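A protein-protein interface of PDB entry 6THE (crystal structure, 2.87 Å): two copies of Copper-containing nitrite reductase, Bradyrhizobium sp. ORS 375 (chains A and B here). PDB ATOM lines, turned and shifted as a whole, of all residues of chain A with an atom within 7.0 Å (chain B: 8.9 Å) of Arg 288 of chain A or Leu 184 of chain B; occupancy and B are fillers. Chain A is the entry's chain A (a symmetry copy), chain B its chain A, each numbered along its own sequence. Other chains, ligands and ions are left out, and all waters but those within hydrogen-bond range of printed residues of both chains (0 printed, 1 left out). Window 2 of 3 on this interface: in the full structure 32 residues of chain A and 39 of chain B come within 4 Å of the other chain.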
ATOM      1  N   PRO A 169       8.601  20.912  -0.836  1.00  0.00           N
ATOM      2  CA  PRO A 169       7.332  20.402  -1.360  1.00  0.00           C
ATOM      3  C   PRO A 169       6.357  20.008  -0.254  1.00  0.00           C
ATOM      4  O   PRO A 169       6.754  19.828   0.896  1.00  0.00           O
ATOM      5  CB  PRO A 169       7.733  19.145  -2.152  1.00  0.00           C
ATOM      6  CG  PRO A 169       9.226  19.282  -2.367  1.00  0.00           C
ATOM      7  CD  PRO A 169       9.730  20.020  -1.146  1.00  0.00           C
ATOM      8  N   TYR A 170       5.077  19.883  -0.628  1.00  0.00           N
ATOM      9  CA  TYR A 170       4.029  19.398   0.255  1.00  0.00           C
ATOM     10  C   TYR A 170       4.366  17.977   0.701  1.00  0.00           C
ATOM     11  O   TYR A 170       4.670  17.120  -0.126  1.00  0.00           O
ATOM     12  CB  TYR A 170       2.674  19.450  -0.459  1.00  0.00           C
ATOM     13  CG  TYR A 170       1.514  18.865   0.309  1.00  0.00           C
ATOM     14  CD1 TYR A 170       1.203  17.516   0.227  1.00  0.00           C
ATOM     15  CD2 TYR A 170       0.712  19.664   1.109  1.00  0.00           C
ATOM     16  CE1 TYR A 170       0.137  16.974   0.930  1.00  0.00           C
ATOM     17  CE2 TYR A 170      -0.357  19.139   1.820  1.00  0.00           C
ATOM     18  CZ  TYR A 170      -0.646  17.789   1.728  1.00  0.00           C
ATOM     19  OH  TYR A 170      -1.699  17.266   2.421  1.00  0.00           O
ATOM     20  N   ARG A 187       1.970  29.052  -7.955  1.00  0.00           N
ATOM     21  CA  ARG A 187       1.940  27.623  -7.688  1.00  0.00           C
ATOM     22  C   ARG A 187       2.183  27.374  -6.202  1.00  0.00           C
ATOM     23  O   ARG A 187       3.301  27.056  -5.800  1.00  0.00           O
ATOM     24  CB  ARG A 187       2.988  26.900  -8.540  1.00  0.00           C
ATOM     25  CG  ARG A 187       2.570  26.683  -9.986  1.00  0.00           C
ATOM     26  CD  ARG A 187       3.470  25.683 -10.682  1.00  0.00           C
ATOM     27  NE  ARG A 187       2.726  25.003 -11.732  1.00  0.00           N
ATOM     28  CZ  ARG A 187       2.097  23.843 -11.579  1.00  0.00           C
ATOM     29  NH1 ARG A 187       2.130  23.212 -10.417  1.00  0.00           N
ATOM     30  NH2 ARG A 187       1.440  23.313 -12.592  1.00  0.00           N
ATOM     31  N   PRO A 188       1.149  27.510  -5.339  1.00  0.00           N
ATOM     32  CA  PRO A 188       1.310  27.256  -3.907  1.00  0.00           C
ATOM     33  C   PRO A 188       1.355  25.762  -3.598  1.00  0.00           C
ATOM     34  O   PRO A 188       0.729  24.960  -4.290  1.00  0.00           O
ATOM     35  CB  PRO A 188       0.070  27.914  -3.284  1.00  0.00           C
ATOM     36  CG  PRO A 188      -0.976  27.868  -4.379  1.00  0.00           C
ATOM     37  CD  PRO A 188      -0.219  27.924  -5.689  1.00  0.00           C
ATOM     38  N   GLU A 189       2.114  25.409  -2.556  1.00  0.00           N
ATOM     39  CA  GLU A 189       2.243  24.030  -2.115  1.00  0.00           C
ATOM     40  C   GLU A 189       1.069  23.678  -1.204  1.00  0.00           C
ATOM     41  O   GLU A 189       0.640  22.527  -1.161  1.00  0.00           O
ATOM     42  CB  GLU A 189       3.577  23.819  -1.394  1.00  0.00           C
ATOM     43  CG  GLU A 189       4.789  23.901  -2.307  1.00  0.00           C
ATOM     44  CD  GLU A 189       5.017  22.711  -3.226  1.00  0.00           C
ATOM     45  OE1 GLU A 189       4.433  21.637  -2.967  1.00  0.00           O
ATOM     46  OE2 GLU A 189       5.781  22.860  -4.199  1.00  0.00           O
ATOM     47  N   TYR A 190       0.560  24.689  -0.488  1.00  0.00           N
ATOM     48  CA  TYR A 190      -0.493  24.500   0.496  1.00  0.00           C
ATOM     49  C   TYR A 190      -1.615  25.507   0.261  1.00  0.00           C
ATOM     50  O   TYR A 190      -1.359  26.684   0.015  1.00  0.00           O
ATOM     51  CB  TYR A 190       0.058  24.677   1.914  1.00  0.00           C
ATOM     52  CG  TYR A 190       1.086  23.661   2.347  1.00  0.00           C
ATOM     53  CD1 TYR A 190       2.428  23.821   2.038  1.00  0.00           C
ATOM     54  CD2 TYR A 190       0.720  22.548   3.087  1.00  0.00           C
ATOM     55  CE1 TYR A 190       3.378  22.894   2.436  1.00  0.00           C
ATOM     56  CE2 TYR A 190       1.657  21.613   3.498  1.00  0.00           C
ATOM     57  CZ  TYR A 190       2.990  21.784   3.169  1.00  0.00           C
ATOM     58  OH  TYR A 190       3.916  20.866   3.569  1.00  0.00           O
ATOM     59  N   PHE A 191      -2.857  25.014   0.334  1.00  0.00           N
ATOM     60  CA  PHE A 191      -4.040  25.849   0.461  1.00  0.00           C
ATOM     61  C   PHE A 191      -4.606  25.657   1.864  1.00  0.00           C
ATOM     62  O   PHE A 191      -4.816  24.526   2.296  1.00  0.00           O
ATOM     63  CB  PHE A 191      -5.078  25.486  -0.604  1.00  0.00           C
ATOM     64  CG  PHE A 191      -4.783  25.992  -1.994  1.00  0.00           C
ATOM     65  CD1 PHE A 191      -5.227  27.240  -2.405  1.00  0.00           C
ATOM     66  CD2 PHE A 191      -4.077  25.212  -2.899  1.00  0.00           C
ATOM     67  CE1 PHE A 191      -4.963  27.703  -3.685  1.00  0.00           C
ATOM     68  CE2 PHE A 191      -3.815  25.674  -4.180  1.00  0.00           C
ATOM     69  CZ  PHE A 191      -4.260  26.917  -4.572  1.00  0.00           C
ATOM     70  N   VAL A 192      -4.840  26.769   2.570  1.00  0.00           N
ATOM     71  CA  VAL A 192      -5.144  26.707   3.992  1.00  0.00           C
ATOM     72  C   VAL A 192      -6.371  27.558   4.313  1.00  0.00           C
ATOM     73  O   VAL A 192      -6.564  28.630   3.740  1.00  0.00           O
ATOM     74  CB  VAL A 192      -3.926  27.106   4.854  1.00  0.00           C
ATOM     75  CG1 VAL A 192      -2.833  26.048   4.822  1.00  0.00           C
ATOM     76  CG2 VAL A 192      -3.366  28.470   4.475  1.00  0.00           C
ATOM     77  N   VAL A 197      -2.864  23.770   7.943  1.00  0.00           N
ATOM     78  CA  VAL A 197      -3.511  22.560   7.464  1.00  0.00           C
ATOM     79  C   VAL A 197      -4.231  21.904   8.640  1.00  0.00           C
ATOM     80  O   VAL A 197      -3.617  21.610   9.665  1.00  0.00           O
ATOM     81  CB  VAL A 197      -2.494  21.601   6.810  1.00  0.00           C
ATOM     82  CG1 VAL A 197      -3.092  20.232   6.521  1.00  0.00           C
ATOM     83  CG2 VAL A 197      -1.885  22.194   5.549  1.00  0.00           C
ATOM     84  N   LEU A 283     -11.399  21.039  -5.858  1.00  0.00           N
ATOM     85  CA  LEU A 283     -11.301  20.064  -4.782  1.00  0.00           C
ATOM     86  C   LEU A 283      -9.960  19.331  -4.784  1.00  0.00           C
ATOM     87  O   LEU A 283      -9.764  18.408  -3.996  1.00  0.00           O
ATOM     88  CB  LEU A 283     -12.483  19.091  -4.867  1.00  0.00           C
ATOM     89  CG  LEU A 283     -13.818  19.625  -4.347  1.00  0.00           C
ATOM     90  CD1 LEU A 283     -14.977  18.780  -4.851  1.00  0.00           C
ATOM     91  CD2 LEU A 283     -13.828  19.687  -2.827  1.00  0.00           C
ATOM     92  N   ALA A 284      -9.037  19.750  -5.658  1.00  0.00           N
ATOM     93  CA  ALA A 284      -7.669  19.259  -5.606  1.00  0.00           C
ATOM     94  C   ALA A 284      -6.916  19.981  -4.492  1.00  0.00           C
ATOM     95  O   ALA A 284      -5.889  19.500  -4.016  1.00  0.00           O
ATOM     96  CB  ALA A 284      -6.993  19.447  -6.941  1.00  0.00           C
ATOM     97  N   ARG A 285      -7.452  21.139  -4.084  1.00  0.00           N
ATOM     98  CA  ARG A 285      -6.874  21.960  -3.034  1.00  0.00           C
ATOM     99  C   ARG A 285      -7.209  21.359  -1.671  1.00  0.00           C
ATOM    100  O   ARG A 285      -6.532  21.645  -0.684  1.00  0.00           O
ATOM    101  CB  ARG A 285      -7.364  23.407  -3.157  1.00  0.00           C
ATOM    102  CG  ARG A 285      -7.072  24.046  -4.508  1.00  0.00           C
ATOM    103  CD  ARG A 285      -7.677  25.425  -4.685  1.00  0.00           C
ATOM    104  NE  ARG A 285      -7.507  25.905  -6.051  1.00  0.00           N
ATOM    105  CZ  ARG A 285      -7.880  27.101  -6.495  1.00  0.00           C
ATOM    106  NH1 ARG A 285      -8.455  27.969  -5.679  1.00  0.00           N
ATOM    107  NH2 ARG A 285      -7.674  27.427  -7.759  1.00  0.00           N
ATOM    108  N   ALA A 286      -8.249  20.515  -1.637  1.00  0.00           N
ATOM    109  CA  ALA A 286      -8.659  19.810  -0.433  1.00  0.00           C
ATOM    110  C   ALA A 286      -7.615  18.761  -0.053  1.00  0.00           C
ATOM    111  O   ALA A 286      -7.592  18.284   1.081  1.00  0.00           O
ATOM    112  CB  ALA A 286     -10.020  19.190  -0.639  1.00  0.00           C
ATOM    113  N   GLU A 287      -6.752  18.415  -1.018  1.00  0.00           N
ATOM    114  CA  GLU A 287      -5.668  17.470  -0.805  1.00  0.00           C
ATOM    115  C   GLU A 287      -4.404  18.225  -0.396  1.00  0.00           C
ATOM    116  O   GLU A 287      -3.365  17.613  -0.154  1.00  0.00           O
ATOM    117  CB  GLU A 287      -5.432  16.637  -2.068  1.00  0.00           C
ATOM    118  CG  GLU A 287      -6.644  15.837  -2.517  1.00  0.00           C
ATOM    119  CD  GLU A 287      -7.083  14.706  -1.600  1.00  0.00           C
ATOM    120  OE1 GLU A 287      -8.278  14.355  -1.633  1.00  0.00           O
ATOM    121  OE2 GLU A 287      -6.229  14.172  -0.860  1.00  0.00           O
ATOM    122  N   ARG A 288      -4.514  19.558  -0.319  1.00  0.00           N
ATOM    123  CA  ARG A 288      -3.387  20.420   0.004  1.00  0.00           C
ATOM    124  C   ARG A 288      -3.680  21.221   1.271  1.00  0.00           C
ATOM    125  O   ARG A 288      -2.998  22.204   1.558  1.00  0.00           O
ATOM    126  CB  ARG A 288      -3.037  21.317  -1.188  1.00  0.00           C
ATOM    127  CG  ARG A 288      -2.409  20.572  -2.357  1.00  0.00           C
ATOM    128  CD  ARG A 288      -1.835  21.487  -3.422  1.00  0.00           C
ATOM    129  NE  ARG A 288      -1.116  20.732  -4.439  1.00  0.00           N
ATOM    130  CZ  ARG A 288       0.179  20.432  -4.396  1.00  0.00           C
ATOM    131  NH1 ARG A 288       0.727  19.735  -5.376  1.00  0.00           N
ATOM    132  NH2 ARG A 288       0.922  20.828  -3.377  1.00  0.00           N
ATOM    133  N   GLY A 289      -4.703  20.791   2.022  1.00  0.00           N
ATOM    134  CA  GLY A 289      -4.965  21.319   3.351  1.00  0.00           C
ATOM    135  C   GLY A 289      -6.241  22.156   3.431  1.00  0.00           C
ATOM    136  O   GLY A 289      -6.671  22.518   4.525  1.00  0.00           O
ATOM    137  N   LEU A 290      -6.835  22.460   2.272  1.00  0.00           N
ATOM    138  CA  LEU A 290      -8.021  23.301   2.212  1.00  0.00           C
ATOM    139  C   LEU A 290      -9.259  22.458   2.512  1.00  0.00           C
ATOM    140  O   LEU A 290      -9.996  22.070   1.607  1.00  0.00           O
ATOM    141  CB  LEU A 290      -8.099  23.965   0.833  1.00  0.00           C
ATOM    142  CG  LEU A 290      -8.948  25.233   0.739  1.00  0.00           C
ATOM    143  CD1 LEU A 290      -8.432  26.312   1.679  1.00  0.00           C
ATOM    144  CD2 LEU A 290      -8.969  25.753  -0.688  1.00  0.00           C
ATOM    145  N   LEU A 291      -9.469  22.191   3.808  1.00  0.00           N
ATOM    146  CA  LEU A 291     -10.556  21.352   4.285  1.00  0.00           C
ATOM    147  C   LEU A 291     -11.015  21.864   5.648  1.00  0.00           C
ATOM    148  O   LEU A 291     -10.196  22.099   6.534  1.00  0.00           O
ATOM    149  CB  LEU A 291     -10.053  19.908   4.384  1.00  0.00           C
ATOM    150  CG  LEU A 291     -11.123  18.838   4.596  1.00  0.00           C
ATOM    151  CD1 LEU A 291     -11.647  18.324   3.263  1.00  0.00           C
ATOM    152  CD2 LEU A 291     -10.573  17.685   5.423  1.00  0.00           C
ATOM    153  N   MET B 129     -10.208   9.617  -3.566  1.00  0.00           N
ATOM    154  CA  MET B 129     -10.162  11.069  -3.490  1.00  0.00           C
ATOM    155  C   MET B 129     -11.148  11.665  -4.492  1.00  0.00           C
ATOM    156  O   MET B 129     -11.235  11.217  -5.635  1.00  0.00           O
ATOM    157  CB  MET B 129      -8.749  11.632  -3.695  1.00  0.00           C
ATOM    158  CG  MET B 129      -8.171  11.437  -5.085  1.00  0.00           C
ATOM    159  SD  MET B 129      -6.832  12.611  -5.438  1.00  0.00           S
ATOM    160  CE  MET B 129      -5.501  11.907  -4.465  1.00  0.00           C
ATOM    161  N   ALA B 131     -11.605  14.511  -6.071  1.00  0.00           N
ATOM    162  CA  ALA B 131     -11.174  15.233  -7.259  1.00  0.00           C
ATOM    163  C   ALA B 131     -10.946  14.270  -8.423  1.00  0.00           C
ATOM    164  O   ALA B 131     -11.166  14.633  -9.576  1.00  0.00           O
ATOM    165  CB  ALA B 131      -9.936  16.037  -6.954  1.00  0.00           C
ATOM    166  N   GLU B 132     -10.509  13.044  -8.104  1.00  0.00           N
ATOM    167  CA  GLU B 132     -10.227  12.017  -9.096  1.00  0.00           C
ATOM    168  C   GLU B 132     -11.534  11.472  -9.670  1.00  0.00           C
ATOM    169  O   GLU B 132     -11.662  11.322 -10.883  1.00  0.00           O
ATOM    170  CB  GLU B 132      -9.376  10.905  -8.477  1.00  0.00           C
ATOM    171  CG  GLU B 132      -9.114   9.738  -9.415  1.00  0.00           C
ATOM    172  CD  GLU B 132      -8.291   8.602  -8.832  1.00  0.00           C
ATOM    173  OE1 GLU B 132      -7.645   7.882  -9.620  1.00  0.00           O
ATOM    174  OE2 GLU B 132      -8.303   8.432  -7.596  1.00  0.00           O
ATOM    175  N   TYR B 165      -7.306  14.546 -16.993  1.00  0.00           N
ATOM    176  CA  TYR B 165      -5.922  14.543 -16.551  1.00  0.00           C
ATOM    177  C   TYR B 165      -5.241  13.261 -17.024  1.00  0.00           C
ATOM    178  O   TYR B 165      -4.903  12.395 -16.219  1.00  0.00           O
ATOM    179  CB  TYR B 165      -5.846  14.720 -15.031  1.00  0.00           C
ATOM    180  CG  TYR B 165      -6.310  16.064 -14.527  1.00  0.00           C
ATOM    181  CD1 TYR B 165      -7.637  16.287 -14.194  1.00  0.00           C
ATOM    182  CD2 TYR B 165      -5.419  17.116 -14.381  1.00  0.00           C
ATOM    183  CE1 TYR B 165      -8.069  17.521 -13.731  1.00  0.00           C
ATOM    184  CE2 TYR B 165      -5.834  18.355 -13.916  1.00  0.00           C
ATOM    185  CZ  TYR B 165      -7.163  18.559 -13.591  1.00  0.00           C
ATOM    186  OH  TYR B 165      -7.576  19.777 -13.136  1.00  0.00           O
ATOM    187  N   PHE B 178      -5.684   8.125 -15.648  1.00  0.00           N
ATOM    188  CA  PHE B 178      -5.682   9.302 -14.795  1.00  0.00           C
ATOM    189  C   PHE B 178      -4.275   9.548 -14.256  1.00  0.00           C
ATOM    190  O   PHE B 178      -3.567   8.606 -13.903  1.00  0.00           O
ATOM    191  CB  PHE B 178      -6.699   9.129 -13.662  1.00  0.00           C
ATOM    192  CG  PHE B 178      -6.728  10.243 -12.647  1.00  0.00           C
ATOM    193  CD1 PHE B 178      -7.471  11.393 -12.873  1.00  0.00           C
ATOM    194  CD2 PHE B 178      -6.021  10.139 -11.458  1.00  0.00           C
ATOM    195  CE1 PHE B 178      -7.499  12.416 -11.936  1.00  0.00           C
ATOM    196  CE2 PHE B 178      -6.048  11.162 -10.522  1.00  0.00           C
ATOM    197  CZ  PHE B 178      -6.789  12.296 -10.763  1.00  0.00           C
ATOM    198  N   SER B 179      -3.887  10.828 -14.204  1.00  0.00           N
ATOM    199  CA  SER B 179      -2.612  11.238 -13.638  1.00  0.00           C
ATOM    200  C   SER B 179      -2.854  12.088 -12.393  1.00  0.00           C
ATOM    201  O   SER B 179      -3.449  13.163 -12.474  1.00  0.00           O
ATOM    202  CB  SER B 179      -1.773  11.969 -14.657  1.00  0.00           C
ATOM    203  OG  SER B 179      -0.498  12.292 -14.122  1.00  0.00           O
ATOM    204  N   VAL B 180      -2.383  11.584 -11.245  1.00  0.00           N
ATOM    205  CA  VAL B 180      -2.576  12.228  -9.955  1.00  0.00           C
ATOM    206  C   VAL B 180      -1.651  13.440  -9.848  1.00  0.00           C
ATOM    207  O   VAL B 180      -1.941  14.382  -9.113  1.00  0.00           O
ATOM    208  CB  VAL B 180      -2.385  11.232  -8.791  1.00  0.00           C
ATOM    209  CG1 VAL B 180      -0.948  10.747  -8.656  1.00  0.00           C
ATOM    210  CG2 VAL B 180      -2.898  11.780  -7.467  1.00  0.00           C
ATOM    211  N   GLU B 181      -0.546  13.406 -10.605  1.00  0.00           N
ATOM    212  CA  GLU B 181       0.451  14.465 -10.608  1.00  0.00           C
ATOM    213  C   GLU B 181      -0.132  15.716 -11.262  1.00  0.00           C
ATOM    214  O   GLU B 181       0.017  16.817 -10.734  1.00  0.00           O
ATOM    215  CB  GLU B 181       1.723  14.006 -11.328  1.00  0.00           C
ATOM    216  CG  GLU B 181       2.478  12.900 -10.607  1.00  0.00           C
ATOM    217  CD  GLU B 181       1.951  11.484 -10.788  1.00  0.00           C
ATOM    218  OE1 GLU B 181       2.509  10.566 -10.153  1.00  0.00           O
ATOM    219  OE2 GLU B 181       0.988  11.297 -11.562  1.00  0.00           O
ATOM    220  N   LYS B 182      -0.797  15.524 -12.409  1.00  0.00           N
ATOM    221  CA  LYS B 182      -1.407  16.605 -13.168  1.00  0.00           C
ATOM    222  C   LYS B 182      -2.585  17.192 -12.393  1.00  0.00           C
ATOM    223  O   LYS B 182      -2.819  18.398 -12.444  1.00  0.00           O
ATOM    224  CB  LYS B 182      -1.867  16.111 -14.544  1.00  0.00           C
ATOM    225  CG  LYS B 182      -0.868  16.278 -15.683  1.00  0.00           C
ATOM    226  CD  LYS B 182       0.104  15.125 -15.829  1.00  0.00           C
ATOM    227  CE  LYS B 182       0.885  15.162 -17.125  1.00  0.00           C
ATOM    228  NZ  LYS B 182       0.032  14.834 -18.294  1.00  0.00           N
ATOM    229  N   LEU B 183      -3.318  16.321 -11.686  1.00  0.00           N
ATOM    230  CA  LEU B 183      -4.503  16.696 -10.929  1.00  0.00           C
ATOM    231  C   LEU B 183      -4.127  17.703  -9.844  1.00  0.00           C
ATOM    232  O   LEU B 183      -4.752  18.757  -9.734  1.00  0.00           O
ATOM    233  CB  LEU B 183      -5.129  15.427 -10.336  1.00  0.00           C
ATOM    234  CG  LEU B 183      -6.482  15.569  -9.630  1.00  0.00           C
ATOM    235  CD1 LEU B 183      -6.320  15.891  -8.153  1.00  0.00           C
ATOM    236  CD2 LEU B 183      -7.394  16.576 -10.319  1.00  0.00           C
ATOM    237  N   LEU B 184      -3.099  17.363  -9.057  1.00  0.00           N
ATOM    238  CA  LEU B 184      -2.649  18.187  -7.946  1.00  0.00           C
ATOM    239  C   LEU B 184      -2.009  19.469  -8.473  1.00  0.00           C
ATOM    240  O   LEU B 184      -2.045  20.499  -7.802  1.00  0.00           O
ATOM    241  CB  LEU B 184      -1.665  17.383  -7.087  1.00  0.00           C
ATOM    242  CG  LEU B 184      -2.263  16.219  -6.298  1.00  0.00           C
ATOM    243  CD1 LEU B 184      -1.170  15.294  -5.784  1.00  0.00           C
ATOM    244  CD2 LEU B 184      -3.124  16.718  -5.146  1.00  0.00           C
ATOM    245  N   ALA B 185      -1.432  19.391  -9.678  1.00  0.00           N
ATOM    246  CA  ALA B 185      -0.805  20.534 -10.322  1.00  0.00           C
ATOM    247  C   ALA B 185      -1.863  21.416 -10.984  1.00  0.00           C
ATOM    248  O   ALA B 185      -1.573  22.553 -11.355  1.00  0.00           O
ATOM    249  CB  ALA B 185       0.228  20.065 -11.318  1.00  0.00           C
ATOM    250  N   GLU B 186      -3.083  20.875 -11.115  1.00  0.00           N
ATOM    251  CA  GLU B 186      -4.206  21.537 -11.767  1.00  0.00           C
ATOM    252  C   GLU B 186      -3.840  21.853 -13.217  1.00  0.00           C
ATOM    253  O   GLU B 186      -4.066  22.964 -13.695  1.00  0.00           O
ATOM    254  CB  GLU B 186      -4.647  22.780 -10.987  1.00  0.00           C
ATOM    255  CG  GLU B 186      -5.304  22.467  -9.654  1.00  0.00           C
ATOM    256  CD  GLU B 186      -5.716  23.677  -8.829  1.00  0.00           C
ATOM    257  OE1 GLU B 186      -6.076  24.712  -9.429  1.00  0.00           O
ATOM    258  OE2 GLU B 186      -5.675  23.582  -7.587  1.00  0.00           O
ATOM    259  N   ARG B 187      -3.275  20.853 -13.904  1.00  0.00           N
ATOM    260  CA  ARG B 187      -2.833  21.000 -15.282  1.00  0.00           C
ATOM    261  C   ARG B 187      -3.463  19.906 -16.141  1.00  0.00           C
ATOM    262  O   ARG B 187      -2.823  18.894 -16.426  1.00  0.00           O
ATOM    263  CB  ARG B 187      -1.304  20.940 -15.359  1.00  0.00           C
ATOM    264  CG  ARG B 187      -0.612  22.232 -14.955  1.00  0.00           C
ATOM    265  CD  ARG B 187       0.846  22.237 -15.370  1.00  0.00           C
ATOM    266  NE  ARG B 187       1.283  23.606 -15.603  1.00  0.00           N
ATOM    267  CZ  ARG B 187       1.278  24.206 -16.787  1.00  0.00           C
ATOM    268  NH1 ARG B 187       0.872  23.557 -17.865  1.00  0.00           N
ATOM    269  NH2 ARG B 187       1.686  25.456 -16.893  1.00  0.00           N
ATOM    270  N   PRO B 188      -4.733  20.070 -16.579  1.00  0.00           N
ATOM    271  CA  PRO B 188      -5.382  19.072 -17.431  1.00  0.00           C
ATOM    272  C   PRO B 188      -4.888  19.150 -18.872  1.00  0.00           C
ATOM    273  O   PRO B 188      -4.535  20.224 -19.357  1.00  0.00           O
ATOM    274  CB  PRO B 188      -6.871  19.435 -17.336  1.00  0.00           C
ATOM    275  CG  PRO B 188      -6.885  20.921 -17.040  1.00  0.00           C
ATOM    276  CD  PRO B 188      -5.611  21.210 -16.273  1.00  0.00           C
ATOM    277  N   PRO B 223     -12.679  19.201 -11.961  1.00  0.00           N
ATOM    278  CA  PRO B 223     -12.991  19.620 -10.593  1.00  0.00           C
ATOM    279  C   PRO B 223     -12.202  20.813 -10.055  1.00  0.00           C
ATOM    280  O   PRO B 223     -12.235  21.073  -8.853  1.00  0.00           O
ATOM    281  CB  PRO B 223     -12.578  18.358  -9.821  1.00  0.00           C
ATOM    282  CG  PRO B 223     -11.348  17.862 -10.559  1.00  0.00           C
ATOM    283  CD  PRO B 223     -11.568  18.238 -12.011  1.00  0.00           C
ATOM    284  N   ASN B 224     -11.514  21.546 -10.941  1.00  0.00           N
ATOM    285  CA  ASN B 224     -10.527  22.518 -10.494  1.00  0.00           C
ATOM    286  C   ASN B 224     -10.800  23.913 -11.057  1.00  0.00           C
ATOM    287  O   ASN B 224     -10.712  24.896 -10.325  1.00  0.00           O
ATOM    288  CB  ASN B 224      -9.097  22.043 -10.768  1.00  0.00           C
ATOM    289  CG  ASN B 224      -8.663  20.931  -9.838  1.00  0.00           C
ATOM    290  OD1 ASN B 224      -9.153  20.825  -8.716  1.00  0.00           O
ATOM    291  ND2 ASN B 224      -7.741  20.097 -10.293  1.00  0.00           N
ATOM    292  N   HIS B 225     -11.117  23.992 -12.354  1.00  0.00           N
ATOM    293  CA  HIS B 225     -11.138  25.270 -13.048  1.00  0.00           C
ATOM    294  C   HIS B 225     -12.566  25.780 -13.230  1.00  0.00           C
ATOM    295  O   HIS B 225     -13.486  25.004 -13.480  1.00  0.00           O
ATOM    296  CB  HIS B 225     -10.362  25.180 -14.369  1.00  0.00           C
ATOM    297  CG  HIS B 225      -8.939  24.771 -14.192  1.00  0.00           C
ATOM    298  ND1 HIS B 225      -7.960  25.660 -13.787  1.00  0.00           N
ATOM    299  CD2 HIS B 225      -8.326  23.579 -14.354  1.00  0.00           C
ATOM    300  CE1 HIS B 225      -6.805  25.031 -13.710  1.00  0.00           C
ATOM    301  NE2 HIS B 225      -7.003  23.753 -14.053  1.00  0.00           N
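CB of Ala 131 of chain B touches O of Leu 283 of chain A (3.8 Å). OD1 of Asn 224 of chain B touches N of Leu 283 of chain A, 3.6 Å away. Leu 183 of chain B touches Ala 284 of chain A. Met 129 of chain B touches Glu 287 of chain A (CB to OE1, 3.4 Å). CD2 of Leu 184 of chain B touches CB of Glu 287 of chain A, 3.8 Å away.
Arg 187 of chain A touches its own counterpart, Arg 187 of chain B. Positions printed for both chains: 187 and 188. Of the 11 pairs that touch across the chains among the printed residues, 1 has its exchanged pair printed and touching as well.
Tyr 190 of chain A touches none of the printed residues of chain B. Of the printed residues of chain B, Leu 283 of chain A touches Ala 131 (3.8 Å), Pro 223 (3.1 Å) and Asn 224 (3.6 Å). Of the printed residues of chain B, Arg 285 of chain A touches Glu 186. Of the printed residues of chain B, Glu 287 of chain A touches Met 129 (3.4 Å) and Leu 184 (3.8 Å). No residue of chain B comes within 4 Å of Gly 289 of chain A. Of the printed residues of chain A, Met 129 of chain B touches Glu 287 (3.4 Å). Of chain A, only Glu 287 (3.8 Å) and Arg 288 (3.5 Å) come within 4 Å of Leu 184 of chain B. Of the printed residues of chain A, Asn 224 of chain B touches Leu 283 and Ala 284. The nearest residue of chain B that does not touch Arg 288 of chain A is Ala 185 of chain B (4.8 Å).
The guanidinium group (NE) of Arg 288 of chain A lies within hydrogen-bond range of the backbone carbonyl oxygen (O) of Leu 184 of chain B (3.5 Å). The side-chain carboxylate (OE2) of Glu 186 of chain B lies within salt-bridge range of the guanidinium group (NE) of Arg 285 of chain A, at 3.3 Å. The guanidinium group (NH2) of Arg 187 of chain A lies within hydrogen-bond range of the backbone carbonyl oxygen (O) of Ala 185 of chain B (3.3 Å). The guanidinium group of Arg 187 of chain A lies close to the guanidinium group of Arg 187 of chain B (3.0 Å). N of Ala 284 of chain A lies close to OD1 of Asn 224 of chain B. The backbone NH of Leu 283 of chain A is in hydrogen-bond range of the backbone carbonyl oxygen of Pro 223 of chain B (3.1 Å).
Of the 18 printed residues of chain B, 9 touch a printed residue of chain A. Hydrophobic or aromatic side chains of chain B that line the printed part of chain A: Met 129, Ala 131, Leu 183, Leu 184 and Ala 185. Hydrophobic or aromatic side chains of chain A within 4 Å of the printed part of chain B: Ala 284. Among the printed residues, Asp or Glu carboxylates within 4 Å of a Lys or Arg side-chain nitrogen of the other chain: Arg 285 of chain A with Glu 186 of chain B (3.3 Å).
The guanidinium group (NH2) of Arg 288 of chain A is in salt-bridge range of the side-chain carboxylate (OE1) of Glu 189 of chain A (3.6 Å). The backbone carbonyl oxygen of Glu 287 of chain A lies within hydrogen-bond range of the side-chain hydroxyl of Tyr 170 of chain A, 3.1 Å away. The side-chain amide nitrogen (ND2) of Asn 224 of chain B sits at hydrogen-bond distance from the side-chain hydroxyl (OH) of Tyr 165 of chain B. The side-chain amide nitrogen (ND2) of Asn 224 of chain B is in hydrogen-bond range of the backbone carbonyl oxygen (O) of Leu 183 of chain B, at 3.3 Å. NE2 of His 225 of chain B is in hydrogen-bond range of O of Glu 186 of chain B (3.1 Å). The backbone carbonyl oxygen (O) of Arg 288 of chain A lies within hydrogen-bond range of the backbone NH (N) of Phe 191 of chain A (3.1 Å).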
